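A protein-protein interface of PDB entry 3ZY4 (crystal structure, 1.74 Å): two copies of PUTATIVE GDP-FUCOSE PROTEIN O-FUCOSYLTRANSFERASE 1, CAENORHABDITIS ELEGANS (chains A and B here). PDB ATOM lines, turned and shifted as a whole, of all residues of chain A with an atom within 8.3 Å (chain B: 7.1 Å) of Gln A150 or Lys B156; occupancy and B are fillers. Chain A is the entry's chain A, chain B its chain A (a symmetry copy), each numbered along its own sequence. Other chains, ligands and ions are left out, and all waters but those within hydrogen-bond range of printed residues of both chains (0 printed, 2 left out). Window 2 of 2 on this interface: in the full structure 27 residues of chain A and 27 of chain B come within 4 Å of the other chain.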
ATOM      1  N   TRP A  99      13.773 -17.702 -15.511  1.00  0.00           N
ATOM      2  CA  TRP A  99      13.210 -18.981 -15.026  1.00  0.00           C
ATOM      3  C   TRP A  99      12.617 -19.844 -16.150  1.00  0.00           C
ATOM      4  O   TRP A  99      12.781 -21.078 -16.166  1.00  0.00           O
ATOM      5  CB  TRP A  99      12.101 -18.709 -14.015  1.00  0.00           C
ATOM      6  CG  TRP A  99      12.573 -18.236 -12.674  1.00  0.00           C
ATOM      7  CD1 TRP A  99      12.866 -16.997 -12.328  1.00  0.00           C
ATOM      8  CD2 TRP A  99      12.843 -19.054 -11.522  1.00  0.00           C
ATOM      9  NE1 TRP A  99      13.262 -16.922 -11.008  1.00  0.00           N
ATOM     10  CE2 TRP A  99      13.257 -18.189 -10.489  1.00  0.00           C
ATOM     11  CE3 TRP A  99      12.763 -20.422 -11.265  1.00  0.00           C
ATOM     12  CZ2 TRP A  99      13.608 -18.654  -9.217  1.00  0.00           C
ATOM     13  CZ3 TRP A  99      13.075 -20.882 -10.004  1.00  0.00           C
ATOM     14  CH2 TRP A  99      13.496 -20.001  -8.992  1.00  0.00           C
ATOM     15  N   ILE A 142      16.537 -26.312 -12.514  1.00  0.00           N
ATOM     16  CA  ILE A 142      17.479 -26.457 -11.416  1.00  0.00           C
ATOM     17  C   ILE A 142      16.680 -26.290 -10.122  1.00  0.00           C
ATOM     18  O   ILE A 142      16.021 -25.276  -9.927  1.00  0.00           O
ATOM     19  CB  ILE A 142      18.578 -25.396 -11.535  1.00  0.00           C
ATOM     20  CG1 ILE A 142      19.299 -25.553 -12.888  1.00  0.00           C
ATOM     21  CG2 ILE A 142      19.489 -25.458 -10.314  1.00  0.00           C
ATOM     22  CD1 ILE A 142      20.350 -24.498 -13.179  1.00  0.00           C
ATOM     23  N   PRO A 143      16.731 -27.274  -9.215  1.00  0.00           N
ATOM     24  CA  PRO A 143      15.807 -27.177  -8.079  1.00  0.00           C
ATOM     25  C   PRO A 143      16.028 -25.909  -7.265  1.00  0.00           C
ATOM     26  O   PRO A 143      17.148 -25.629  -6.865  1.00  0.00           O
ATOM     27  CB  PRO A 143      16.095 -28.471  -7.267  1.00  0.00           C
ATOM     28  CG  PRO A 143      17.335 -29.053  -7.850  1.00  0.00           C
ATOM     29  CD  PRO A 143      17.481 -28.540  -9.241  1.00  0.00           C
ATOM     30  N   GLY A 144      14.969 -25.112  -7.095  1.00  0.00           N
ATOM     31  CA  GLY A 144      15.055 -23.834  -6.400  1.00  0.00           C
ATOM     32  C   GLY A 144      15.567 -22.676  -7.256  1.00  0.00           C
ATOM     33  O   GLY A 144      15.715 -21.568  -6.751  1.00  0.00           O
ATOM     34  N   GLY A 145      15.849 -22.926  -8.534  1.00  0.00           N
ATOM     35  CA  GLY A 145      16.469 -21.902  -9.411  1.00  0.00           C
ATOM     36  C   GLY A 145      17.798 -21.379  -8.855  1.00  0.00           C
ATOM     37  O   GLY A 145      18.794 -22.126  -8.741  1.00  0.00           O
ATOM     38  N   PHE A 146      17.814 -20.099  -8.470  1.00  0.00           N
ATOM     39  CA  PHE A 146      19.026 -19.487  -7.913  1.00  0.00           C
ATOM     40  C   PHE A 146      19.163 -19.634  -6.390  1.00  0.00           C
ATOM     41  O   PHE A 146      20.074 -19.060  -5.797  1.00  0.00           O
ATOM     42  CB  PHE A 146      19.100 -17.985  -8.322  1.00  0.00           C
ATOM     43  CG  PHE A 146      17.820 -17.230  -8.081  1.00  0.00           C
ATOM     44  CD1 PHE A 146      17.301 -17.087  -6.788  1.00  0.00           C
ATOM     45  CD2 PHE A 146      17.131 -16.647  -9.150  1.00  0.00           C
ATOM     46  CE1 PHE A 146      16.084 -16.389  -6.556  1.00  0.00           C
ATOM     47  CE2 PHE A 146      15.948 -15.952  -8.938  1.00  0.00           C
ATOM     48  CZ  PHE A 146      15.416 -15.811  -7.652  1.00  0.00           C
ATOM     49  N   ASP A 147      18.296 -20.416  -5.746  1.00  0.00           N
ATOM     50  CA  ASP A 147      18.358 -20.519  -4.286  1.00  0.00           C
ATOM     51  C   ASP A 147      19.630 -21.204  -3.760  1.00  0.00           C
ATOM     52  O   ASP A 147      20.223 -20.762  -2.759  1.00  0.00           O
ATOM     53  CB  ASP A 147      17.107 -21.184  -3.737  1.00  0.00           C
ATOM     54  CG  ASP A 147      15.917 -20.267  -3.763  1.00  0.00           C
ATOM     55  OD1 ASP A 147      16.116 -19.073  -4.064  1.00  0.00           O
ATOM     56  OD2 ASP A 147      14.794 -20.740  -3.478  1.00  0.00           O
ATOM     57  N   LEU A 148      20.051 -22.261  -4.443  1.00  0.00           N
ATOM     58  CA  LEU A 148      21.217 -23.071  -4.022  1.00  0.00           C
ATOM     59  C   LEU A 148      20.943 -23.669  -2.654  1.00  0.00           C
ATOM     60  O   LEU A 148      21.849 -23.961  -1.868  1.00  0.00           O
ATOM     61  CB  LEU A 148      22.507 -22.241  -4.040  1.00  0.00           C
ATOM     62  CG  LEU A 148      22.872 -21.720  -5.428  1.00  0.00           C
ATOM     63  CD1 LEU A 148      24.254 -21.197  -5.396  1.00  0.00           C
ATOM     64  CD2 LEU A 148      22.761 -22.827  -6.474  1.00  0.00           C
ATOM     65  N   ASN A 149      19.658 -23.882  -2.422  1.00  0.00           N
ATOM     66  CA  ASN A 149      19.090 -24.237  -1.149  1.00  0.00           C
ATOM     67  C   ASN A 149      18.954 -25.736  -1.062  1.00  0.00           C
ATOM     68  O   ASN A 149      18.742 -26.298   0.016  1.00  0.00           O
ATOM     69  CB  ASN A 149      17.689 -23.625  -1.082  1.00  0.00           C
ATOM     70  CG  ASN A 149      17.397 -22.996   0.251  1.00  0.00           C
ATOM     71  OD1 ASN A 149      18.086 -23.252   1.234  1.00  0.00           O
ATOM     72  ND2 ASN A 149      16.372 -22.163   0.296  1.00  0.00           N
ATOM     73  N   GLN A 150      19.055 -26.376  -2.223  1.00  0.00           N
ATOM     74  CA  GLN A 150      18.631 -27.752  -2.384  1.00  0.00           C
ATOM     75  C   GLN A 150      19.757 -28.621  -2.897  1.00  0.00           C
ATOM     76  O   GLN A 150      20.645 -28.156  -3.609  1.00  0.00           O
ATOM     77  CB  GLN A 150      17.422 -27.829  -3.314  1.00  0.00           C
ATOM     78  CG  GLN A 150      16.310 -26.881  -2.905  1.00  0.00           C
ATOM     79  CD  GLN A 150      15.014 -27.093  -3.667  1.00  0.00           C
ATOM     80  OE1 GLN A 150      14.722 -28.186  -4.157  1.00  0.00           O
ATOM     81  NE2 GLN A 150      14.219 -26.040  -3.753  1.00  0.00           N
ATOM     82  N   MET A 151      19.697 -29.894  -2.536  1.00  0.00           N
ATOM     83  CA  MET A 151      20.781 -30.824  -2.789  1.00  0.00           C
ATOM     84  C   MET A 151      20.932 -31.074  -4.284  1.00  0.00           C
ATOM     85  O   MET A 151      19.978 -31.451  -4.964  1.00  0.00           O
ATOM     86  CB  MET A 151      20.533 -32.127  -2.009  1.00  0.00           C
ATOM     87  CG  MET A 151      20.720 -32.006  -0.471  1.00  0.00           C
ATOM     88  SD  MET A 151      20.089 -30.487   0.322  1.00  0.00           S
ATOM     89  CE  MET A 151      19.479 -31.144   1.878  1.00  0.00           C
ATOM     90  N   GLY A 152      22.133 -30.830  -4.796  1.00  0.00           N
ATOM     91  CA  GLY A 152      22.410 -30.997  -6.224  1.00  0.00           C
ATOM     92  C   GLY A 152      22.179 -29.750  -7.068  1.00  0.00           C
ATOM     93  O   GLY A 152      22.516 -29.741  -8.254  1.00  0.00           O
ATOM     94  N   SER A 153      21.603 -28.707  -6.466  1.00  0.00           N
ATOM     95  CA  SER A 153      21.320 -27.432  -7.169  1.00  0.00           C
ATOM     96  C   SER A 153      22.576 -26.703  -7.626  1.00  0.00           C
ATOM     97  O   SER A 153      22.688 -26.295  -8.781  1.00  0.00           O
ATOM     98  CB  SER A 153      20.502 -26.506  -6.279  1.00  0.00           C
ATOM     99  OG  SER A 153      19.142 -26.892  -6.267  1.00  0.00           O
ATOM    100  N   ARG A 154      23.524 -26.538  -6.707  1.00  0.00           N
ATOM    101  CA  ARG A 154      24.813 -25.933  -7.017  1.00  0.00           C
ATOM    102  C   ARG A 154      25.484 -26.663  -8.192  1.00  0.00           C
ATOM    103  O   ARG A 154      25.939 -26.047  -9.153  1.00  0.00           O
ATOM    104  CB  ARG A 154      25.696 -25.993  -5.768  1.00  0.00           C
ATOM    105  CG  ARG A 154      26.567 -24.782  -5.528  1.00  0.00           C
ATOM    106  CD  ARG A 154      27.871 -25.190  -4.832  1.00  0.00           C
ATOM    107  NE  ARG A 154      29.003 -24.395  -5.310  1.00  0.00           N
ATOM    108  CZ  ARG A 154      29.737 -24.689  -6.384  1.00  0.00           C
ATOM    109  NH1 ARG A 154      29.478 -25.777  -7.100  1.00  0.00           N
ATOM    110  NH2 ARG A 154      30.739 -23.895  -6.742  1.00  0.00           N
ATOM    111  N   LYS A 155      25.527 -27.989  -8.107  1.00  0.00           N
ATOM    112  CA  LYS A 155      26.182 -28.826  -9.112  1.00  0.00           C
ATOM    113  C   LYS A 155      25.472 -28.811 -10.465  1.00  0.00           C
ATOM    114  O   LYS A 155      26.113 -28.913 -11.518  1.00  0.00           O
ATOM    115  CB  LYS A 155      26.282 -30.267  -8.597  1.00  0.00           C
ATOM    116  CG  LYS A 155      27.690 -30.847  -8.588  1.00  0.00           C
ATOM    117  CD  LYS A 155      28.648 -30.042  -7.703  1.00  0.00           C
ATOM    118  CE  LYS A 155      29.533 -30.961  -6.857  1.00  0.00           C
ATOM    119  NZ  LYS A 155      30.472 -31.833  -7.633  1.00  0.00           N
ATOM    120  N   LYS A 156      24.149 -28.696 -10.435  1.00  0.00           N
ATOM    121  CA  LYS A 156      23.367 -28.586 -11.664  1.00  0.00           C
ATOM    122  C   LYS A 156      23.678 -27.279 -12.397  1.00  0.00           C
ATOM    123  O   LYS A 156      23.759 -27.264 -13.620  1.00  0.00           O
ATOM    124  CB  LYS A 156      21.869 -28.714 -11.391  1.00  0.00           C
ATOM    125  CG  LYS A 156      21.380 -30.152 -11.321  1.00  0.00           C
ATOM    126  CD  LYS A 156      19.856 -30.226 -11.430  1.00  0.00           C
ATOM    127  CE  LYS A 156      19.389 -31.678 -11.436  1.00  0.00           C
ATOM    128  NZ  LYS A 156      17.922 -31.817 -11.178  1.00  0.00           N
ATOM    129  N   TRP A 157      23.868 -26.191 -11.655  1.00  0.00           N
ATOM    130  CA  TRP A 157      24.342 -24.956 -12.269  1.00  0.00           C
ATOM    131  C   TRP A 157      25.673 -25.176 -13.002  1.00  0.00           C
ATOM    132  O   TRP A 157      25.826 -24.762 -14.152  1.00  0.00           O
ATOM    133  CB  TRP A 157      24.483 -23.850 -11.226  1.00  0.00           C
ATOM    134  CG  TRP A 157      23.211 -23.114 -10.974  1.00  0.00           C
ATOM    135  CD1 TRP A 157      22.362 -23.288  -9.926  1.00  0.00           C
ATOM    136  CD2 TRP A 157      22.668 -22.045 -11.765  1.00  0.00           C
ATOM    137  NE1 TRP A 157      21.295 -22.419 -10.024  1.00  0.00           N
ATOM    138  CE2 TRP A 157      21.463 -21.632 -11.136  1.00  0.00           C
ATOM    139  CE3 TRP A 157      23.075 -21.402 -12.942  1.00  0.00           C
ATOM    140  CZ2 TRP A 157      20.653 -20.606 -11.650  1.00  0.00           C
ATOM    141  CZ3 TRP A 157      22.255 -20.364 -13.458  1.00  0.00           C
ATOM    142  CH2 TRP A 157      21.064 -19.993 -12.806  1.00  0.00           C
ATOM    143  N   LYS A 183      19.534 -15.129   6.570  1.00  0.00           N
ATOM    144  CA  LYS A 183      20.929 -15.537   6.354  1.00  0.00           C
ATOM    145  C   LYS A 183      21.784 -14.569   5.512  1.00  0.00           C
ATOM    146  O   LYS A 183      23.020 -14.604   5.586  1.00  0.00           O
ATOM    147  CB  LYS A 183      20.987 -16.938   5.745  1.00  0.00           C
ATOM    148  CG  LYS A 183      20.117 -17.153   4.532  1.00  0.00           C
ATOM    149  CD  LYS A 183      20.031 -18.635   4.171  1.00  0.00           C
ATOM    150  CE  LYS A 183      19.013 -18.889   3.052  1.00  0.00           C
ATOM    151  NZ  LYS A 183      19.521 -19.830   1.999  1.00  0.00           N
ATOM    152  N   GLY B 140       8.597 -21.508  -7.634  1.00  0.00           N
ATOM    153  CA  GLY B 140       9.986 -21.708  -8.048  1.00  0.00           C
ATOM    154  C   GLY B 140      10.785 -22.627  -7.126  1.00  0.00           C
ATOM    155  O   GLY B 140      11.725 -23.236  -7.589  1.00  0.00           O
ATOM    156  N   ASP B 141      10.445 -22.712  -5.838  1.00  0.00           N
ATOM    157  CA  ASP B 141      11.201 -23.589  -4.909  1.00  0.00           C
ATOM    158  C   ASP B 141      10.797 -25.071  -4.946  1.00  0.00           C
ATOM    159  O   ASP B 141      11.450 -25.922  -4.327  1.00  0.00           O
ATOM    160  CB  ASP B 141      11.222 -23.058  -3.469  1.00  0.00           C
ATOM    161  CG  ASP B 141       9.857 -23.072  -2.810  1.00  0.00           C
ATOM    162  OD1 ASP B 141       8.953 -23.736  -3.342  1.00  0.00           O
ATOM    163  OD2 ASP B 141       9.690 -22.421  -1.752  1.00  0.00           O
ATOM    164  N   ILE B 142       9.730 -25.368  -5.679  1.00  0.00           N
ATOM    165  CA  ILE B 142       9.393 -26.753  -5.962  1.00  0.00           C
ATOM    166  C   ILE B 142      10.306 -27.206  -7.104  1.00  0.00           C
ATOM    167  O   ILE B 142      10.321 -26.594  -8.165  1.00  0.00           O
ATOM    168  CB  ILE B 142       7.915 -26.857  -6.353  1.00  0.00           C
ATOM    169  CG1 ILE B 142       7.042 -26.313  -5.205  1.00  0.00           C
ATOM    170  CG2 ILE B 142       7.594 -28.284  -6.782  1.00  0.00           C
ATOM    171  CD1 ILE B 142       5.555 -26.265  -5.501  1.00  0.00           C
ATOM    172  N   PRO B 143      11.072 -28.288  -6.913  1.00  0.00           N
ATOM    173  CA  PRO B 143      12.073 -28.582  -7.944  1.00  0.00           C
ATOM    174  C   PRO B 143      11.442 -28.811  -9.311  1.00  0.00           C
ATOM    175  O   PRO B 143      10.528 -29.613  -9.433  1.00  0.00           O
ATOM    176  CB  PRO B 143      12.796 -29.844  -7.397  1.00  0.00           C
ATOM    177  CG  PRO B 143      11.975 -30.322  -6.250  1.00  0.00           C
ATOM    178  CD  PRO B 143      11.172 -29.174  -5.742  1.00  0.00           C
ATOM    179  N   GLY B 144      11.882 -28.045 -10.312  1.00  0.00           N
ATOM    180  CA  GLY B 144      11.315 -28.107 -11.653  1.00  0.00           C
ATOM    181  C   GLY B 144      10.029 -27.305 -11.841  1.00  0.00           C
ATOM    182  O   GLY B 144       9.451 -27.327 -12.922  1.00  0.00           O
ATOM    183  N   GLN B 150      10.803 -34.383 -11.141  1.00  0.00           N
ATOM    184  CA  GLN B 150      11.843 -34.567 -10.149  1.00  0.00           C
ATOM    185  C   GLN B 150      11.290 -35.145  -8.867  1.00  0.00           C
ATOM    186  O   GLN B 150      10.131 -34.925  -8.519  1.00  0.00           O
ATOM    187  CB  GLN B 150      12.560 -33.245  -9.882  1.00  0.00           C
ATOM    188  CG  GLN B 150      13.029 -32.566 -11.156  1.00  0.00           C
ATOM    189  CD  GLN B 150      13.937 -31.374 -10.916  1.00  0.00           C
ATOM    190  OE1 GLN B 150      14.623 -31.277  -9.895  1.00  0.00           O
ATOM    191  NE2 GLN B 150      13.956 -30.463 -11.874  1.00  0.00           N
ATOM    192  N   MET B 151      12.142 -35.875  -8.163  1.00  0.00           N
ATOM    193  CA  MET B 151      11.730 -36.646  -7.005  1.00  0.00           C
ATOM    194  C   MET B 151      11.312 -35.721  -5.869  1.00  0.00           C
ATOM    195  O   MET B 151      12.068 -34.841  -5.457  1.00  0.00           O
ATOM    196  CB  MET B 151      12.868 -37.594  -6.588  1.00  0.00           C
ATOM    197  CG  MET B 151      13.105 -38.786  -7.556  1.00  0.00           C
ATOM    198  SD  MET B 151      12.996 -38.434  -9.345  1.00  0.00           S
ATOM    199  CE  MET B 151      14.289 -39.504  -9.982  1.00  0.00           C
ATOM    200  N   GLY B 152      10.088 -35.907  -5.388  1.00  0.00           N
ATOM    201  CA  GLY B 152       9.547 -35.070  -4.317  1.00  0.00           C
ATOM    202  C   GLY B 152       8.795 -33.833  -4.793  1.00  0.00           C
ATOM    203  O   GLY B 152       8.180 -33.138  -3.982  1.00  0.00           O
ATOM    204  N   SER B 153       8.849 -33.555  -6.098  1.00  0.00           N
ATOM    205  CA  SER B 153       8.164 -32.383  -6.697  1.00  0.00           C
ATOM    206  C   SER B 153       6.647 -32.452  -6.590  1.00  0.00           C
ATOM    207  O   SER B 153       5.997 -31.500  -6.159  1.00  0.00           O
ATOM    208  CB  SER B 153       8.555 -32.231  -8.160  1.00  0.00           C
ATOM    209  OG  SER B 153       9.836 -31.643  -8.279  1.00  0.00           O
ATOM    210  N   ARG B 154       6.083 -33.588  -6.994  1.00  0.00           N
ATOM    211  CA  ARG B 154       4.651 -33.831  -6.876  1.00  0.00           C
ATOM    212  C   ARG B 154       4.184 -33.616  -5.427  1.00  0.00           C
ATOM    213  O   ARG B 154       3.208 -32.915  -5.166  1.00  0.00           O
ATOM    214  CB  ARG B 154       4.358 -35.262  -7.331  1.00  0.00           C
ATOM    215  CG  ARG B 154       3.080 -35.447  -8.118  1.00  0.00           C
ATOM    216  CD  ARG B 154       2.488 -36.837  -7.857  1.00  0.00           C
ATOM    217  NE  ARG B 154       1.025 -36.796  -7.824  1.00  0.00           N
ATOM    218  CZ  ARG B 154       0.298 -36.520  -6.740  1.00  0.00           C
ATOM    219  NH1 ARG B 154       0.890 -36.272  -5.577  1.00  0.00           N
ATOM    220  NH2 ARG B 154      -1.027 -36.497  -6.816  1.00  0.00           N
ATOM    221  N   LYS B 155       4.903 -34.218  -4.486  1.00  0.00           N
ATOM    222  CA  LYS B 155       4.557 -34.162  -3.066  1.00  0.00           C
ATOM    223  C   LYS B 155       4.709 -32.766  -2.463  1.00  0.00           C
ATOM    224  O   LYS B 155       3.955 -32.380  -1.562  1.00  0.00           O
ATOM    225  CB  LYS B 155       5.421 -35.159  -2.284  1.00  0.00           C
ATOM    226  CG  LYS B 155       4.640 -36.165  -1.449  1.00  0.00           C
ATOM    227  CD  LYS B 155       3.707 -37.033  -2.301  1.00  0.00           C
ATOM    228  CE  LYS B 155       3.766 -38.502  -1.877  1.00  0.00           C
ATOM    229  NZ  LYS B 155       3.284 -38.784  -0.488  1.00  0.00           N
ATOM    230  N   LYS B 156       5.690 -32.016  -2.954  1.00  0.00           N
ATOM    231  CA  LYS B 156       5.882 -30.636  -2.518  1.00  0.00           C
ATOM    232  C   LYS B 156       4.706 -29.756  -2.948  1.00  0.00           C
ATOM    233  O   LYS B 156       4.277 -28.890  -2.193  1.00  0.00           O
ATOM    234  CB  LYS B 156       7.205 -30.064  -3.027  1.00  0.00           C
ATOM    235  CG  LYS B 156       8.398 -30.407  -2.149  1.00  0.00           C
ATOM    236  CD  LYS B 156       9.600 -29.518  -2.473  1.00  0.00           C
ATOM    237  CE  LYS B 156      10.762 -29.823  -1.533  1.00  0.00           C
ATOM    238  NZ  LYS B 156      12.062 -29.262  -2.015  1.00  0.00           N
ATOM    239  N   TRP B 157       4.177 -29.985  -4.146  1.00  0.00           N
ATOM    240  CA  TRP B 157       2.948 -29.310  -4.549  1.00  0.00           C
ATOM    241  C   TRP B 157       1.812 -29.585  -3.552  1.00  0.00           C
ATOM    242  O   TRP B 157       1.130 -28.658  -3.115  1.00  0.00           O
ATOM    243  CB  TRP B 157       2.535 -29.727  -5.957  1.00  0.00           C
ATOM    244  CG  TRP B 157       3.199 -28.928  -7.026  1.00  0.00           C
ATOM    245  CD1 TRP B 157       4.266 -29.304  -7.782  1.00  0.00           C
ATOM    246  CD2 TRP B 157       2.806 -27.628  -7.495  1.00  0.00           C
ATOM    247  NE1 TRP B 157       4.594 -28.306  -8.676  1.00  0.00           N
ATOM    248  CE2 TRP B 157       3.706 -27.271  -8.534  1.00  0.00           C
ATOM    249  CE3 TRP B 157       1.790 -26.732  -7.137  1.00  0.00           C
ATOM    250  CZ2 TRP B 157       3.626 -26.045  -9.216  1.00  0.00           C
ATOM    251  CZ3 TRP B 157       1.710 -25.496  -7.830  1.00  0.00           C
ATOM    252  CH2 TRP B 157       2.630 -25.178  -8.848  1.00  0.00           C
ATOM    253  N   LEU B 158       1.625 -30.857  -3.201  1.00  0.00           N
ATOM    254  CA  LEU B 158       0.579 -31.256  -2.243  1.00  0.00           C
ATOM    255  C   LEU B 158       0.799 -30.670  -0.855  1.00  0.00           C
ATOM    256  O   LEU B 158      -0.145 -30.234  -0.191  1.00  0.00           O
ATOM    257  CB  LEU B 158       0.451 -32.779  -2.186  1.00  0.00           C
ATOM    258  CG  LEU B 158      -0.620 -33.409  -3.098  1.00  0.00           C
ATOM    259  CD1 LEU B 158      -0.167 -33.518  -4.561  1.00  0.00           C
ATOM    260  CD2 LEU B 158      -1.045 -34.776  -2.551  1.00  0.00           C
ATOM    261  N   GLU B 159       2.063 -30.637  -0.447  1.00  0.00           N
ATOM    262  CA  GLU B 159       2.496 -30.151   0.849  1.00  0.00           C
ATOM    263  C   GLU B 159       2.351 -28.644   0.946  1.00  0.00           C
ATOM    264  O   GLU B 159       1.838 -28.120   1.931  1.00  0.00           O
ATOM    265  CB  GLU B 159       3.963 -30.561   1.065  1.00  0.00           C
ATOM    266  CG  GLU B 159       4.800 -29.588   1.877  1.00  0.00           C
ATOM    267  CD  GLU B 159       6.100 -30.191   2.374  1.00  0.00           C
ATOM    268  OE1 GLU B 159       6.890 -30.723   1.559  1.00  0.00           O
ATOM    269  OE2 GLU B 159       6.326 -30.123   3.591  1.00  0.00           O
ATOM    270  N   LYS B 160       2.783 -27.950  -0.106  1.00  0.00           N
ATOM    271  CA  LYS B 160       2.886 -26.516  -0.056  1.00  0.00           C
ATOM    272  C   LYS B 160       1.536 -25.843  -0.295  1.00  0.00           C
ATOM    273  O   LYS B 160       1.235 -24.820   0.307  1.00  0.00           O
ATOM    274  CB  LYS B 160       3.907 -26.049  -1.091  1.00  0.00           C
ATOM    275  CG  LYS B 160       4.141 -24.604  -1.067  1.00  0.00           C
ATOM    276  CD  LYS B 160       5.275 -24.234  -1.996  1.00  0.00           C
ATOM    277  CE  LYS B 160       5.786 -22.869  -1.613  1.00  0.00           C
ATOM    278  NZ  LYS B 160       6.628 -22.338  -2.714  1.00  0.00           N
ATOM    279  N   PHE B 161       0.722 -26.437  -1.166  1.00  0.00           N
ATOM    280  CA  PHE B 161      -0.562 -25.846  -1.531  1.00  0.00           C
ATOM    281  C   PHE B 161      -1.717 -26.828  -1.327  1.00  0.00           C
ATOM    282  O   PHE B 161      -2.320 -27.285  -2.301  1.00  0.00           O
ATOM    283  CB  PHE B 161      -0.517 -25.314  -2.973  1.00  0.00           C
ATOM    284  CG  PHE B 161       0.557 -24.282  -3.193  1.00  0.00           C
ATOM    285  CD1 PHE B 161       0.513 -23.084  -2.503  1.00  0.00           C
ATOM    286  CD2 PHE B 161       1.607 -24.517  -4.079  1.00  0.00           C
ATOM    287  CE1 PHE B 161       1.484 -22.122  -2.663  1.00  0.00           C
ATOM    288  CE2 PHE B 161       2.598 -23.540  -4.267  1.00  0.00           C
ATOM    289  CZ  PHE B 161       2.537 -22.346  -3.562  1.00  0.00           C
ATOM    290  N   PRO B 162      -2.034 -27.135  -0.056  1.00  0.00           N
ATOM    291  CA  PRO B 162      -3.112 -28.106   0.207  1.00  0.00           C
ATOM    292  C   PRO B 162      -4.472 -27.558  -0.225  1.00  0.00           C
ATOM    293  O   PRO B 162      -4.708 -26.342  -0.145  1.00  0.00           O
ATOM    294  CB  PRO B 162      -3.055 -28.307   1.730  1.00  0.00           C
ATOM    295  CG  PRO B 162      -1.779 -27.644   2.196  1.00  0.00           C
ATOM    296  CD  PRO B 162      -1.463 -26.591   1.187  1.00  0.00           C
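The side-chain amide nitrogen of Gln A150 lies within hydrogen-bond range of the backbone carbonyl oxygen of Asp B141.
The backbone carbonyl oxygen (O) of Pro A143 is in hydrogen-bond range of the side-chain hydroxyl (OG) of Ser A153 (2.4 Å).
The backbone carbonyl oxygen (O) of Gln A150 lies close to the side-chain hydroxyl (OG) of Ser A153 (3.3 Å).
The side-chain carboxylate (OD1) of Asp B141 lies within salt-bridge range of the side-chain amino group (NZ) of Lys B160 (2.8 Å).
The side-chain hydroxyl of Ser B153 is in hydrogen-bond range of the backbone carbonyl oxygen of Pro B143, 2.4 Å away.
O of Gln B150 lies close to OG of Ser B153.
Among the printed residues, merely in contact across the chains: Pro A143 with Pro B143, Lys A156 with Gln B150, Gln A150 with Lys B156, Gly A144 with Gly B140 and Trp A99 with Gly B140.
Of the printed residues of chain B, Gln A150 touches Asp B141 and Lys B156.
Of chain A, only Gln A150 (3.6 Å) comes within 4 Å of Lys B156.
Of the printed residues of chain B, Pro A143 touches Pro B143.
Of the printed residues of chain B, Gly A144 touches Gly B140.
Printed residues of chain B within 4 Å of Trp A99: Gly B140.
Lys B155 touches none of the printed residues of chain A.
The nearest printed residue of chain B that does not touch Gln A150 is Pro B143 (4.01 Å).
The nearest printed residue of chain B that does not touch Gly A144 is Asp B141 (4.1 Å).
Of the 18 printed residues of chain A, 5 touch a printed residue of chain B.
Printed residues of chain A that touch a printed residue of chain B: Trp A99, Pro A143, Gly A144, Gln A150 and Lys A156.
Hydrophobic or aromatic side chains of chain A within 4 Å of the printed part of chain B: Trp A99 and Pro A143.
Printed residues of chain B that touch a printed residue of chain A: Gly B140, Asp B141, Pro B143, Gln B150 and Lys B156.
Hydrophobic or aromatic side chains of chain B within 4 Å of the printed part of chain A: Pro B143.
Among the printed residues, 6 pairs touch across the chains.
Among the printed residues, no Asp or Glu carboxylate lies within 4 Å of a Lys or Arg side-chain nitrogen of the other chain.
Pro A143 touches its own counterpart, Pro B143.
Gln A150 touches Lys B156, and with the chains exchanged Lys A156 touches Gln B150.
11 positions are printed for both chains.
Of the 6 pairs that touch across the chains among the printed residues, 3 have their exchanged pair printed and touching as well.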
